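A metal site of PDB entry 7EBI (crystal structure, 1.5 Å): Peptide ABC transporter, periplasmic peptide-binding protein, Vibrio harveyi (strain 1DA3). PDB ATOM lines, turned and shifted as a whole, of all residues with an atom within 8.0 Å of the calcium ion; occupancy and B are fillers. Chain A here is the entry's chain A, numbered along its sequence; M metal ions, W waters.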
ATOM      1  N   LYS A 339      -5.758  19.760   6.351  1.00  0.00           N
ATOM      2  CA  LYS A 339      -6.686  19.607   5.255  1.00  0.00           C
ATOM      3  C   LYS A 339      -6.535  20.767   4.294  1.00  0.00           C
ATOM      4  O   LYS A 339      -6.428  21.913   4.723  1.00  0.00           O
ATOM      5  CB  LYS A 339      -8.107  19.525   5.799  1.00  0.00           C
ATOM      6  CG  LYS A 339      -9.198  19.460   4.740  1.00  0.00           C
ATOM      7  CD  LYS A 339     -10.563  19.396   5.406  1.00  0.00           C
ATOM      8  CE  LYS A 339     -11.681  19.487   4.386  1.00  0.00           C
ATOM      9  NZ  LYS A 339     -13.013  19.616   5.070  1.00  0.00           N
ATOM     10  N   ASP A 340      -6.530  20.467   3.001  1.00  0.00           N
ATOM     11  CA  ASP A 340      -6.558  21.517   1.972  1.00  0.00           C
ATOM     12  C   ASP A 340      -7.950  22.127   1.887  1.00  0.00           C
ATOM     13  O   ASP A 340      -8.899  21.446   1.483  1.00  0.00           O
ATOM     14  CB  ASP A 340      -6.150  20.949   0.612  1.00  0.00           C
ATOM     15  CG  ASP A 340      -6.178  21.992  -0.488  1.00  0.00           C
ATOM     16  OD1 ASP A 340      -6.042  23.196  -0.176  1.00  0.00           O
ATOM     17  OD2 ASP A 340      -6.353  21.609  -1.671  1.00  0.00           O
ATOM     18  N   VAL A 341      -8.075  23.399   2.261  1.00  0.00           N
ATOM     19  CA  VAL A 341      -9.370  24.061   2.237  1.00  0.00           C
ATOM     20  C   VAL A 341      -9.435  25.227   1.255  1.00  0.00           C
ATOM     21  O   VAL A 341     -10.424  25.963   1.251  1.00  0.00           O
ATOM     22  CB  VAL A 341      -9.780  24.548   3.648  1.00  0.00           C
ATOM     23  CG1 VAL A 341     -10.054  23.352   4.557  1.00  0.00           C
ATOM     24  CG2 VAL A 341      -8.728  25.463   4.255  1.00  0.00           C
ATOM     25  N   ASN A 342      -8.430  25.369   0.389  1.00  0.00           N
ATOM     26  CA  ASN A 342      -8.531  26.377  -0.682  1.00  0.00           C
ATOM     27  C   ASN A 342      -8.145  25.846  -2.069  1.00  0.00           C
ATOM     28  O   ASN A 342      -7.720  26.601  -2.942  1.00  0.00           O
ATOM     29  CB  ASN A 342      -7.722  27.643  -0.329  1.00  0.00           C
ATOM     30  CG  ASN A 342      -6.235  27.410  -0.239  1.00  0.00           C
ATOM     31  OD1 ASN A 342      -5.755  26.286  -0.249  1.00  0.00           O
ATOM     32  ND2 ASN A 342      -5.475  28.505  -0.137  1.00  0.00           N
ATOM     33  N   LYS A 343      -8.334  24.546  -2.262  1.00  0.00           N
ATOM     34  CA  LYS A 343      -8.326  23.919  -3.591  1.00  0.00           C
ATOM     35  C   LYS A 343      -7.046  24.110  -4.391  1.00  0.00           C
ATOM     36  O   LYS A 343      -7.105  24.217  -5.614  1.00  0.00           O
ATOM     37  CB  LYS A 343      -9.508  24.448  -4.428  1.00  0.00           C
ATOM     38  CG  LYS A 343     -10.863  24.335  -3.749  1.00  0.00           C
ATOM     39  CD  LYS A 343     -11.942  24.865  -4.674  1.00  0.00           C
ATOM     40  CE  LYS A 343     -13.272  24.907  -3.969  1.00  0.00           C
ATOM     41  NZ  LYS A 343     -13.201  25.807  -2.783  1.00  0.00           N
ATOM     42  N   ASP A 344      -5.891  24.154  -3.736  1.00  0.00           N
ATOM     43  CA  ASP A 344      -4.638  24.269  -4.484  1.00  0.00           C
ATOM     44  C   ASP A 344      -3.794  23.007  -4.387  1.00  0.00           C
ATOM     45  O   ASP A 344      -2.685  22.935  -4.929  1.00  0.00           O
ATOM     46  CB  ASP A 344      -3.843  25.510  -4.023  1.00  0.00           C
ATOM     47  CG  ASP A 344      -3.265  25.379  -2.623  1.00  0.00           C
ATOM     48  OD1 ASP A 344      -3.659  24.478  -1.844  1.00  0.00           O
ATOM     49  OD2 ASP A 344      -2.386  26.227  -2.290  1.00  0.00           O
ATOM     50  N   GLY A 345      -4.303  21.993  -3.697  1.00  0.00           N
ATOM     51  CA  GLY A 345      -3.630  20.715  -3.627  1.00  0.00           C
ATOM     52  C   GLY A 345      -2.626  20.624  -2.495  1.00  0.00           C
ATOM     53  O   GLY A 345      -2.007  19.582  -2.306  1.00  0.00           O
ATOM     54  N   PHE A 346      -2.492  21.707  -1.735  1.00  0.00           N
ATOM     55  CA  PHE A 346      -1.535  21.728  -0.621  1.00  0.00           C
ATOM     56  C   PHE A 346      -2.267  21.840   0.715  1.00  0.00           C
ATOM     57  O   PHE A 346      -3.169  22.664   0.873  1.00  0.00           O
ATOM     58  CB  PHE A 346      -0.531  22.860  -0.784  1.00  0.00           C
ATOM     59  CG  PHE A 346       0.388  22.682  -1.982  1.00  0.00           C
ATOM     60  CD1 PHE A 346       1.346  21.683  -1.989  1.00  0.00           C
ATOM     61  CD2 PHE A 346       0.275  23.504  -3.080  1.00  0.00           C
ATOM     62  CE1 PHE A 346       2.170  21.497  -3.085  1.00  0.00           C
ATOM     63  CE2 PHE A 346       1.099  23.336  -4.190  1.00  0.00           C
ATOM     64  CZ  PHE A 346       2.053  22.331  -4.190  1.00  0.00           C
ATOM     65  N   VAL A 347      -1.872  21.022   1.679  1.00  0.00           N
ATOM     66  CA  VAL A 347      -2.561  21.011   2.954  1.00  0.00           C
ATOM     67  C   VAL A 347      -2.393  22.339   3.661  1.00  0.00           C
ATOM     68  O   VAL A 347      -1.393  23.046   3.485  1.00  0.00           O
ATOM     69  CB  VAL A 347      -2.085  19.861   3.882  1.00  0.00           C
ATOM     70  CG1 VAL A 347      -2.282  18.514   3.200  1.00  0.00           C
ATOM     71  CG2 VAL A 347      -0.624  20.062   4.294  1.00  0.00           C
ATOM     72  N   ASP A 348      -3.404  22.710   4.434  1.00  0.00           N
ATOM     73  CA  ASP A 348      -3.377  23.908   5.240  1.00  0.00           C
ATOM     74  C   ASP A 348      -3.381  23.493   6.712  1.00  0.00           C
ATOM     75  O   ASP A 348      -3.601  22.327   7.019  1.00  0.00           O
ATOM     76  CB  ASP A 348      -4.569  24.788   4.851  1.00  0.00           C
ATOM     77  CG  ASP A 348      -4.594  25.020   3.319  1.00  0.00           C
ATOM     78  OD1 ASP A 348      -3.555  25.483   2.798  1.00  0.00           O
ATOM     79  OD2 ASP A 348      -5.591  24.696   2.628  1.00  0.00           O
ATOM     80  N   THR A 349      -3.089  24.421   7.613  1.00  0.00           N
ATOM     81  CA  THR A 349      -3.023  24.071   9.021  1.00  0.00           C
ATOM     82  C   THR A 349      -4.408  23.751   9.568  1.00  0.00           C
ATOM     83  O   THR A 349      -5.408  24.099   8.948  1.00  0.00           O
ATOM     84  CB  THR A 349      -2.435  25.201   9.865  1.00  0.00           C
ATOM     85  OG1 THR A 349      -3.343  26.310   9.881  1.00  0.00           O
ATOM     86  CG2 THR A 349      -1.078  25.624   9.306  1.00  0.00           C
ATOM     87  N   GLY A 352      -6.758  26.498   9.468  1.00  0.00           N
ATOM     88  CA  GLY A 352      -7.198  26.884   8.132  1.00  0.00           C
ATOM     89  C   GLY A 352      -6.220  27.719   7.326  1.00  0.00           C
ATOM     90  O   GLY A 352      -6.572  28.214   6.258  1.00  0.00           O
ATOM     91  N   LYS A 353      -4.997  27.850   7.824  1.00  0.00           N
ATOM     92  CA  LYS A 353      -4.034  28.754   7.189  1.00  0.00           C
ATOM     93  C   LYS A 353      -3.157  28.048   6.167  1.00  0.00           C
ATOM     94  O   LYS A 353      -2.659  26.949   6.396  1.00  0.00           O
ATOM     95  CB  LYS A 353      -3.145  29.407   8.246  1.00  0.00           C
ATOM     96  CG  LYS A 353      -3.857  30.270   9.281  1.00  0.00           C
ATOM     97  CD  LYS A 353      -2.851  30.790  10.297  1.00  0.00           C
ATOM     98  CE  LYS A 353      -3.524  31.613  11.407  1.00  0.00           C
ATOM     99  NZ  LYS A 353      -4.428  30.780  12.242  1.00  0.00           N
ATOM    100  N   SER A 354      -2.968  28.699   5.025  1.00  0.00           N
ATOM    101  CA  SER A 354      -2.026  28.206   4.024  1.00  0.00           C
ATOM    102  C   SER A 354      -0.619  28.566   4.448  1.00  0.00           C
ATOM    103  O   SER A 354      -0.398  29.526   5.186  1.00  0.00           O
ATOM    104  CB  SER A 354      -2.334  28.807   2.654  1.00  0.00           C
ATOM    105  OG  SER A 354      -3.569  28.327   2.164  1.00  0.00           O
ATOM    106  N   PHE A 355       0.345  27.781   3.978  1.00  0.00           N
ATOM    107  CA  PHE A 355       1.733  28.032   4.290  1.00  0.00           C
ATOM    108  C   PHE A 355       2.639  27.340   3.293  1.00  0.00           C
ATOM    109  O   PHE A 355       2.256  26.347   2.656  1.00  0.00           O
ATOM    110  CB  PHE A 355       2.066  27.568   5.714  1.00  0.00           C
ATOM    111  CG  PHE A 355       1.959  26.082   5.904  1.00  0.00           C
ATOM    112  CD1 PHE A 355       0.734  25.478   6.173  1.00  0.00           C
ATOM    113  CD2 PHE A 355       3.089  25.284   5.837  1.00  0.00           C
ATOM    114  CE1 PHE A 355       0.641  24.094   6.361  1.00  0.00           C
ATOM    115  CE2 PHE A 355       3.006  23.911   6.024  1.00  0.00           C
ATOM    116  CZ  PHE A 355       1.772  23.314   6.280  1.00  0.00           C
ATOM    117  N   GLY A 383       1.337  16.706  -0.669  1.00  0.00           N
ATOM    118  CA  GLY A 383       0.567  17.909  -0.431  1.00  0.00           C
ATOM    119  C   GLY A 383       1.167  18.877   0.561  1.00  0.00           C
ATOM    120  O   GLY A 383       0.462  19.743   1.069  1.00  0.00           O
ATOM    121  N   LYS A 385       3.572  22.016   0.891  1.00  0.00           N
ATOM    122  CA  LYS A 385       4.142  23.054   0.025  1.00  0.00           C
ATOM    123  C   LYS A 385       5.454  23.547   0.606  1.00  0.00           C
ATOM    124  O   LYS A 385       5.499  23.972   1.760  1.00  0.00           O
ATOM    125  CB  LYS A 385       3.160  24.206  -0.144  1.00  0.00           C
ATOM    126  CG  LYS A 385       3.522  25.140  -1.288  1.00  0.00           C
ATOM    127  CD  LYS A 385       2.461  26.203  -1.534  1.00  0.00           C
ATOM    128  CE  LYS A 385       2.758  26.993  -2.800  1.00  0.00           C
ATOM    129  NZ  LYS A 385       1.671  27.965  -3.135  1.00  0.00           N
HETATM  130 CA    CA M   1      -4.326  24.672   0.501  1.00  0.00          CA
HETATM  131  O   HOH W   1      -2.401  26.046   0.333  1.00  0.00           O
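The side-chain carboxylate (OD2) of Asp 348 lies close to the backbone NH (N) of Val 341, 2.8 Å away.
The backbone NH (N) of Lys 343 lies close to the side-chain carboxylate (OD1) of Asp 340 (3.4 Å).
The side-chain carboxylate (OD1) of Asp 348 lies close to the side-chain hydroxyl (OG) of Ser 354, at 2.9 Å.
ND2 of Asn 342 is in hydrogen-bond range of OG of Ser 354 (3.0 Å).
The side-chain carboxylate of Asp 340 lies within hydrogen-bond range of the backbone NH of Gly 345 (2.9 Å).
The backbone carbonyl oxygen of Lys 339 lies within hydrogen-bond range of the backbone NH of Asp 348 (3.1 Å).
Water W1 lies within hydrogen-bond range of OD2 of Asp 344 (2.6 Å) and OG of Ser 354 (3.1 Å).
The calcium ion is bound by OD1 of Asn 342 (2.3 Å), O of Phe 346 (2.3 Å), OD1 of Asp 340 (2.4 Å), water W1 (2.4 Å), OD1 of Asp 344 (2.4 Å), OD2 of Asp 348 (2.5 Å) and OD1 of Asp 348 (2.6 Å).
The calcium ion has seven donor atoms within binding distance.
Of the 17 residues printed, 5 come within 4 Å of the calcium ion.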
